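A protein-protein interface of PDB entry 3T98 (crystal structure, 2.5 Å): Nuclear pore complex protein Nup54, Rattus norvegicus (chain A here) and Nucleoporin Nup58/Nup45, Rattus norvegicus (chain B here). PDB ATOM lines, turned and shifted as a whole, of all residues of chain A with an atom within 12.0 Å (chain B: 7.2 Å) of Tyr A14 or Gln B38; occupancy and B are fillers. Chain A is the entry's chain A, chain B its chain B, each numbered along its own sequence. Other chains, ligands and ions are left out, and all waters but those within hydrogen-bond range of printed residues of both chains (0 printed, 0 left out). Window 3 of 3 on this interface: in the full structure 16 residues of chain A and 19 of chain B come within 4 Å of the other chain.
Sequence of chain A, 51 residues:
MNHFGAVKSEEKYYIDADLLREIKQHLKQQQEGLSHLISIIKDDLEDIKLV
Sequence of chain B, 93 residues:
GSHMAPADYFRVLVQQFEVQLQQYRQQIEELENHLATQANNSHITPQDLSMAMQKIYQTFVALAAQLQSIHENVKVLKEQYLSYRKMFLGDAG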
ATOM      1  N   TYR A  13       4.631  -7.043 -31.965  1.00  0.00           N
ATOM      2  CA  TYR A  13       3.870  -5.793 -31.691  1.00  0.00           C
ATOM      3  C   TYR A  13       3.392  -5.674 -30.237  1.00  0.00           C
ATOM      4  O   TYR A  13       4.143  -5.211 -29.372  1.00  0.00           O
ATOM      5  CB  TYR A  13       2.691  -5.668 -32.676  1.00  0.00           C
ATOM      6  CG  TYR A  13       2.077  -6.989 -33.131  1.00  0.00           C
ATOM      7  CD1 TYR A  13       1.238  -7.728 -32.289  1.00  0.00           C
ATOM      8  CD2 TYR A  13       2.338  -7.498 -34.406  1.00  0.00           C
ATOM      9  CE1 TYR A  13       0.675  -8.939 -32.705  1.00  0.00           C
ATOM     10  CE2 TYR A  13       1.782  -8.710 -34.833  1.00  0.00           C
ATOM     11  CZ  TYR A  13       0.954  -9.423 -33.976  1.00  0.00           C
ATOM     12  OH  TYR A  13       0.408 -10.619 -34.380  1.00  0.00           O
ATOM     13  N   TYR A  14       2.160  -6.108 -29.971  1.00  0.00           N
ATOM     14  CA  TYR A  14       1.566  -6.047 -28.629  1.00  0.00           C
ATOM     15  C   TYR A  14       0.950  -7.385 -28.207  1.00  0.00           C
ATOM     16  O   TYR A  14       1.157  -8.412 -28.855  1.00  0.00           O
ATOM     17  CB  TYR A  14       0.484  -4.966 -28.591  1.00  0.00           C
ATOM     18  CG  TYR A  14      -0.372  -4.956 -29.833  1.00  0.00           C
ATOM     19  CD1 TYR A  14       0.002  -4.210 -30.951  1.00  0.00           C
ATOM     20  CD2 TYR A  14      -1.537  -5.721 -29.907  1.00  0.00           C
ATOM     21  CE1 TYR A  14      -0.765  -4.223 -32.116  1.00  0.00           C
ATOM     22  CE2 TYR A  14      -2.311  -5.743 -31.066  1.00  0.00           C
ATOM     23  CZ  TYR A  14      -1.918  -4.988 -32.165  1.00  0.00           C
ATOM     24  OH  TYR A  14      -2.686  -4.983 -33.307  1.00  0.00           O
ATOM     25  N   ILE A  15       0.176  -7.354 -27.125  1.00  0.00           N
ATOM     26  CA  ILE A  15      -0.474  -8.553 -26.594  1.00  0.00           C
ATOM     27  C   ILE A  15      -2.011  -8.503 -26.671  1.00  0.00           C
ATOM     28  O   ILE A  15      -2.597  -7.431 -26.838  1.00  0.00           O
ATOM     29  CB  ILE A  15      -0.056  -8.796 -25.122  1.00  0.00           C
ATOM     30  CG1 ILE A  15      -0.413  -7.579 -24.264  1.00  0.00           C
ATOM     31  CG2 ILE A  15       1.440  -9.090 -25.055  1.00  0.00           C
ATOM     32  CD1 ILE A  15      -0.176  -7.765 -22.772  1.00  0.00           C
ATOM     33  N   ASP A  16      -2.652  -9.669 -26.545  1.00  0.00           N
ATOM     34  CA  ASP A  16      -4.117  -9.790 -26.601  1.00  0.00           C
ATOM     35  C   ASP A  16      -4.835  -8.720 -25.795  1.00  0.00           C
ATOM     36  O   ASP A  16      -4.391  -8.338 -24.712  1.00  0.00           O
ATOM     37  CB  ASP A  16      -4.566 -11.156 -26.068  1.00  0.00           C
ATOM     38  CG  ASP A  16      -3.986 -12.310 -26.850  1.00  0.00           C
ATOM     39  OD1 ASP A  16      -4.444 -12.545 -27.988  1.00  0.00           O
ATOM     40  OD2 ASP A  16      -3.068 -12.978 -26.324  1.00  0.00           O
ATOM     41  N   ALA A  17      -5.964  -8.259 -26.320  1.00  0.00           N
ATOM     42  CA  ALA A  17      -6.764  -7.253 -25.635  1.00  0.00           C
ATOM     43  C   ALA A  17      -7.326  -7.867 -24.353  1.00  0.00           C
ATOM     44  O   ALA A  17      -7.703  -7.146 -23.423  1.00  0.00           O
ATOM     45  CB  ALA A  17      -7.901  -6.776 -26.534  1.00  0.00           C
ATOM     46  N   ASP A  18      -7.381  -9.199 -24.310  1.00  0.00           N
ATOM     47  CA  ASP A  18      -7.888  -9.897 -23.131  1.00  0.00           C
ATOM     48  C   ASP A  18      -6.761 -10.371 -22.218  1.00  0.00           C
ATOM     49  O   ASP A  18      -6.981 -10.612 -21.031  1.00  0.00           O
ATOM     50  CB  ASP A  18      -8.787 -11.079 -23.528  1.00  0.00           C
ATOM     51  CG  ASP A  18      -8.077 -12.100 -24.393  1.00  0.00           C
ATOM     52  OD1 ASP A  18      -6.983 -12.569 -23.998  1.00  0.00           O
ATOM     53  OD2 ASP A  18      -8.626 -12.444 -25.464  1.00  0.00           O
ATOM     54  N   LEU A  19      -5.561 -10.517 -22.769  1.00  0.00           N
ATOM     55  CA  LEU A  19      -4.421 -10.917 -21.958  1.00  0.00           C
ATOM     56  C   LEU A  19      -4.124  -9.692 -21.107  1.00  0.00           C
ATOM     57  O   LEU A  19      -3.639  -9.792 -19.978  1.00  0.00           O
ATOM     58  CB  LEU A  19      -3.221 -11.253 -22.841  1.00  0.00           C
ATOM     59  CG  LEU A  19      -1.871 -11.546 -22.176  1.00  0.00           C
ATOM     60  CD1 LEU A  19      -2.041 -12.281 -20.857  1.00  0.00           C
ATOM     61  CD2 LEU A  19      -1.037 -12.369 -23.141  1.00  0.00           C
ATOM     62  N   LEU A  20      -4.436  -8.529 -21.666  1.00  0.00           N
ATOM     63  CA  LEU A  20      -4.249  -7.279 -20.964  1.00  0.00           C
ATOM     64  C   LEU A  20      -5.214  -7.285 -19.781  1.00  0.00           C
ATOM     65  O   LEU A  20      -4.822  -7.008 -18.646  1.00  0.00           O
ATOM     66  CB  LEU A  20      -4.560  -6.105 -21.894  1.00  0.00           C
ATOM     67  CG  LEU A  20      -4.562  -4.717 -21.242  1.00  0.00           C
ATOM     68  CD1 LEU A  20      -3.184  -4.416 -20.667  1.00  0.00           C
ATOM     69  CD2 LEU A  20      -4.961  -3.661 -22.264  1.00  0.00           C
ATOM     70  N   ARG A  21      -6.474  -7.615 -20.070  1.00  0.00           N
ATOM     71  CA  ARG A  21      -7.553  -7.694 -19.085  1.00  0.00           C
ATOM     72  C   ARG A  21      -7.232  -8.645 -17.939  1.00  0.00           C
ATOM     73  O   ARG A  21      -7.558  -8.376 -16.784  1.00  0.00           O
ATOM     74  CB  ARG A  21      -8.844  -8.135 -19.769  1.00  0.00           C
ATOM     75  CG  ARG A  21      -9.912  -7.057 -19.785  1.00  0.00           C
ATOM     76  CD  ARG A  21     -10.582  -6.939 -21.147  1.00  0.00           C
ATOM     77  NE  ARG A  21     -11.405  -8.099 -21.474  1.00  0.00           N
ATOM     78  CZ  ARG A  21     -11.973  -8.295 -22.659  1.00  0.00           C
ATOM     79  NH1 ARG A  21     -11.801  -7.404 -23.631  1.00  0.00           N
ATOM     80  NH2 ARG A  21     -12.713  -9.378 -22.874  1.00  0.00           N
ATOM     81  N   ILE A  23      -4.166  -9.516 -16.832  1.00  0.00           N
ATOM     82  CA  ILE A  23      -3.124  -8.889 -16.029  1.00  0.00           C
ATOM     83  C   ILE A  23      -3.697  -7.753 -15.185  1.00  0.00           C
ATOM     84  O   ILE A  23      -3.369  -7.607 -14.009  1.00  0.00           O
ATOM     85  CB  ILE A  23      -2.012  -8.323 -16.941  1.00  0.00           C
ATOM     86  CG1 ILE A  23      -1.325  -9.473 -17.687  1.00  0.00           C
ATOM     87  CG2 ILE A  23      -1.016  -7.521 -16.123  1.00  0.00           C
ATOM     88  CD1 ILE A  23      -0.354  -9.022 -18.769  1.00  0.00           C
ATOM     89  N   LYS A  24      -4.550  -6.946 -15.800  1.00  0.00           N
ATOM     90  CA  LYS A  24      -5.168  -5.817 -15.123  1.00  0.00           C
ATOM     91  C   LYS A  24      -6.009  -6.330 -13.953  1.00  0.00           C
ATOM     92  O   LYS A  24      -6.128  -5.680 -12.907  1.00  0.00           O
ATOM     93  CB  LYS A  24      -6.027  -5.048 -16.126  1.00  0.00           C
ATOM     94  CG  LYS A  24      -6.541  -3.709 -15.641  1.00  0.00           C
ATOM     95  CD  LYS A  24      -7.044  -2.863 -16.819  1.00  0.00           C
ATOM     96  CE  LYS A  24      -5.897  -2.445 -17.756  1.00  0.00           C
ATOM     97  NZ  LYS A  24      -6.374  -1.650 -18.940  1.00  0.00           N
ATOM     98  N   HIS B  34       3.990   0.583 -19.547  1.00  0.00           N
ATOM     99  CA  HIS B  34       4.229  -0.366 -20.631  1.00  0.00           C
ATOM    100  C   HIS B  34       2.934  -0.892 -21.236  1.00  0.00           C
ATOM    101  O   HIS B  34       2.891  -1.257 -22.410  1.00  0.00           O
ATOM    102  CB  HIS B  34       5.077  -1.546 -20.147  1.00  0.00           C
ATOM    103  CG  HIS B  34       6.466  -1.167 -19.742  1.00  0.00           C
ATOM    104  ND1 HIS B  34       7.147  -0.110 -20.311  1.00  0.00           N
ATOM    105  CD2 HIS B  34       7.315  -1.716 -18.839  1.00  0.00           C
ATOM    106  CE1 HIS B  34       8.350  -0.022 -19.774  1.00  0.00           C
ATOM    107  NE2 HIS B  34       8.477  -0.986 -18.878  1.00  0.00           N
ATOM    108  N   LEU B  35       1.877  -0.925 -20.435  1.00  0.00           N
ATOM    109  CA  LEU B  35       0.594  -1.407 -20.910  1.00  0.00           C
ATOM    110  C   LEU B  35      -0.366  -0.256 -21.163  1.00  0.00           C
ATOM    111  O   LEU B  35      -1.529  -0.473 -21.505  1.00  0.00           O
ATOM    112  CB  LEU B  35      -0.010  -2.385 -19.896  1.00  0.00           C
ATOM    113  CG  LEU B  35       0.842  -3.626 -19.616  1.00  0.00           C
ATOM    114  CD1 LEU B  35       0.047  -4.634 -18.804  1.00  0.00           C
ATOM    115  CD2 LEU B  35       1.285  -4.252 -20.931  1.00  0.00           C
ATOM    116  N   ALA B  36       0.126   0.969 -21.005  1.00  0.00           N
ATOM    117  CA  ALA B  36      -0.696   2.159 -21.212  1.00  0.00           C
ATOM    118  C   ALA B  36      -1.206   2.258 -22.648  1.00  0.00           C
ATOM    119  O   ALA B  36      -2.328   2.711 -22.892  1.00  0.00           O
ATOM    120  CB  ALA B  36       0.098   3.406 -20.855  1.00  0.00           C
ATOM    121  N   THR B  37      -0.377   1.839 -23.598  1.00  0.00           N
ATOM    122  CA  THR B  37      -0.750   1.884 -25.006  1.00  0.00           C
ATOM    123  C   THR B  37      -0.002   0.817 -25.788  1.00  0.00           C
ATOM    124  O   THR B  37       0.932   0.199 -25.276  1.00  0.00           O
ATOM    125  CB  THR B  37      -0.425   3.258 -25.641  1.00  0.00           C
ATOM    126  OG1 THR B  37       0.974   3.528 -25.505  1.00  0.00           O
ATOM    127  CG2 THR B  37      -1.218   4.370 -24.964  1.00  0.00           C
ATOM    128  N   GLN B  38      -0.423   0.603 -27.031  1.00  0.00           N
ATOM    129  CA  GLN B  38       0.224  -0.376 -27.893  1.00  0.00           C
ATOM    130  C   GLN B  38       1.522   0.224 -28.424  1.00  0.00           C
ATOM    131  O   GLN B  38       2.439  -0.502 -28.809  1.00  0.00           O
ATOM    132  CB  GLN B  38      -0.685  -0.741 -29.062  1.00  0.00           C
ATOM    133  CG  GLN B  38      -1.992  -1.375 -28.653  1.00  0.00           C
ATOM    134  CD  GLN B  38      -2.891  -1.638 -29.842  1.00  0.00           C
ATOM    135  OE1 GLN B  38      -3.218  -0.724 -30.598  1.00  0.00           O
ATOM    136  NE2 GLN B  38      -3.297  -2.892 -30.014  1.00  0.00           N
ATOM    137  N   ALA B  39       1.588   1.553 -28.445  1.00  0.00           N
ATOM    138  CA  ALA B  39       2.773   2.262 -28.918  1.00  0.00           C
ATOM    139  C   ALA B  39       3.946   2.011 -27.967  1.00  0.00           C
ATOM    140  O   ALA B  39       5.087   1.837 -28.400  1.00  0.00           O
ATOM    141  CB  ALA B  39       2.485   3.758 -29.014  1.00  0.00           C
ATOM    142  N   ASN B  40       3.652   1.987 -26.671  1.00  0.00           N
ATOM    143  CA  ASN B  40       4.672   1.761 -25.656  1.00  0.00           C
ATOM    144  C   ASN B  40       4.883   0.269 -25.465  1.00  0.00           C
ATOM    145  O   ASN B  40       5.960  -0.174 -25.064  1.00  0.00           O
ATOM    146  CB  ASN B  40       4.242   2.380 -24.326  1.00  0.00           C
ATOM    147  CG  ASN B  40       3.656   3.767 -24.493  1.00  0.00           C
ATOM    148  OD1 ASN B  40       4.153   4.573 -25.283  1.00  0.00           O
ATOM    149  ND2 ASN B  40       2.600   4.057 -23.739  1.00  0.00           N
ATOM    150  N   ASN B  41       3.835  -0.494 -25.759  1.00  0.00           N
ATOM    151  CA  ASN B  41       3.852  -1.947 -25.625  1.00  0.00           C
ATOM    152  C   ASN B  41       4.766  -2.596 -26.675  1.00  0.00           C
ATOM    153  O   ASN B  41       5.271  -3.704 -26.477  1.00  0.00           O
ATOM    154  CB  ASN B  41       2.416  -2.476 -25.762  1.00  0.00           C
ATOM    155  CG  ASN B  41       2.261  -3.917 -25.288  1.00  0.00           C
ATOM    156  OD1 ASN B  41       1.158  -4.474 -25.319  1.00  0.00           O
ATOM    157  ND2 ASN B  41       3.360  -4.524 -24.844  1.00  0.00           N
ATOM    158  N   SER B  42       4.984  -1.893 -27.784  1.00  0.00           N
ATOM    159  CA  SER B  42       5.823  -2.392 -28.872  1.00  0.00           C
ATOM    160  C   SER B  42       7.314  -2.312 -28.555  1.00  0.00           C
ATOM    161  O   SER B  42       8.131  -2.919 -29.244  1.00  0.00           O
ATOM    162  CB  SER B  42       5.543  -1.601 -30.148  1.00  0.00           C
ATOM    163  OG  SER B  42       5.864  -0.232 -29.962  1.00  0.00           O
ATOM    164  N   HIS B  43       7.667  -1.556 -27.522  1.00  0.00           N
ATOM    165  CA  HIS B  43       9.064  -1.413 -27.127  1.00  0.00           C
ATOM    166  C   HIS B  43       9.424  -2.476 -26.096  1.00  0.00           C
ATOM    167  O   HIS B  43      10.547  -2.518 -25.601  1.00  0.00           O
ATOM    168  CB  HIS B  43       9.304  -0.020 -26.546  1.00  0.00           C
ATOM    169  CG  HIS B  43       8.880   1.093 -27.455  1.00  0.00           C
ATOM    170  ND1 HIS B  43       8.894   2.417 -27.068  1.00  0.00           N
ATOM    171  CD2 HIS B  43       8.421   1.079 -28.729  1.00  0.00           C
ATOM    172  CE1 HIS B  43       8.458   3.169 -28.063  1.00  0.00           C
ATOM    173  NE2 HIS B  43       8.166   2.381 -29.083  1.00  0.00           N
ATOM    174  N   ILE B  44       8.457  -3.339 -25.791  1.00  0.00           N
ATOM    175  CA  ILE B  44       8.638  -4.413 -24.821  1.00  0.00           C
ATOM    176  C   ILE B  44       8.200  -5.738 -25.446  1.00  0.00           C
ATOM    177  O   ILE B  44       7.536  -5.756 -26.473  1.00  0.00           O
ATOM    178  CB  ILE B  44       7.785  -4.155 -23.548  1.00  0.00           C
ATOM    179  CG1 ILE B  44       8.375  -4.902 -22.356  1.00  0.00           C
ATOM    180  CG2 ILE B  44       6.352  -4.630 -23.759  1.00  0.00           C
ATOM    181  CD1 ILE B  44       9.657  -4.302 -21.849  1.00  0.00           C
ATOM    182  N   PRO B  46       6.605  -9.928 -24.759  1.00  0.00           N
ATOM    183  CA  PRO B  46       5.739 -10.683 -23.852  1.00  0.00           C
ATOM    184  C   PRO B  46       6.561 -11.476 -22.833  1.00  0.00           C
ATOM    185  O   PRO B  46       6.015 -12.123 -21.937  1.00  0.00           O
ATOM    186  CB  PRO B  46       4.956 -11.584 -24.806  1.00  0.00           C
ATOM    187  CG  PRO B  46       5.966 -11.853 -25.897  1.00  0.00           C
ATOM    188  CD  PRO B  46       6.534 -10.470 -26.130  1.00  0.00           C
ATOM    189  N   LEU B  49       7.182  -8.574 -19.860  1.00  0.00           N
ATOM    190  CA  LEU B  49       6.011  -8.453 -19.009  1.00  0.00           C
ATOM    191  C   LEU B  49       6.040  -9.661 -18.091  1.00  0.00           C
ATOM    192  O   LEU B  49       5.861  -9.540 -16.887  1.00  0.00           O
ATOM    193  CB  LEU B  49       4.737  -8.481 -19.845  1.00  0.00           C
ATOM    194  CG  LEU B  49       4.488  -7.305 -20.787  1.00  0.00           C
ATOM    195  CD1 LEU B  49       3.271  -7.611 -21.655  1.00  0.00           C
ATOM    196  CD2 LEU B  49       4.266  -6.036 -19.991  1.00  0.00           C
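The backbone carbonyl oxygen (O) of Ala B39 sits at hydrogen-bond distance from the side-chain hydroxyl (OG) of Ser B42, at 2.7 Å.
The backbone carbonyl oxygen (O) of Asn B41 lies close to the backbone carbonyl oxygen (O) of Tyr A13 (3.5 Å).
Tyr A14 touches two residues of chain B.
Gln B38 touches one residue of chain A.
No residue of chain A comes within 4 Å of Ala B36.
No residue of chain A comes within 4 Å of Thr B37.
No residue of chain A comes within 4 Å of Asn B40.
Asn B41 touches just these residues of chain A: Tyr A13, Tyr A14 and Ile A15.
Printed residues of chain B within 4 Å of Leu A20: Leu B35 (3.7 Å).
Printed residues of chain B within 4 Å of Tyr A13: Asn B41 (3.5 Å) and Ser B42 (3.3 Å).
Of the printed residues of chain A, Leu B35 touches Leu A20 (3.7 Å).
Arg A21 touches none of the printed residues of chain B.
Among the printed residues, pairs that only touch across the chains: Tyr A14 with Gln B38 (3.2 Å), Tyr A13 with Ser B42 (3.3 Å), Tyr A14 with Asn B41 (3.4 Å), Ile A15 with Asn B41 (3.5 Å), Ile A15 with Leu B49 (3.6 Å) and Leu A20 with Leu B35 (3.7 Å).
Of the 11 printed residues of chain A, 4 touch a printed residue of chain B.
Hydrophobic or aromatic side chains of chain A within 4 Å of the printed part of chain B: Tyr A14, Ile A15 and Leu A20.
Of the 13 printed residues of chain B, 5 touch a printed residue of chain A.
Printed residues of chain B that touch a printed residue of chain A: Leu B35, Gln B38, Asn B41, Ser B42 and Leu B49.
Hydrophobic or aromatic side chains of chain B within 4 Å of the printed part of chain A: Leu B35 and Leu B49.
Among the printed residues, 7 pairs touch across the chains.
Among the printed residues, no Asp or Glu carboxylate lies within 4 Å of a Lys or Arg side-chain nitrogen of the other chain.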
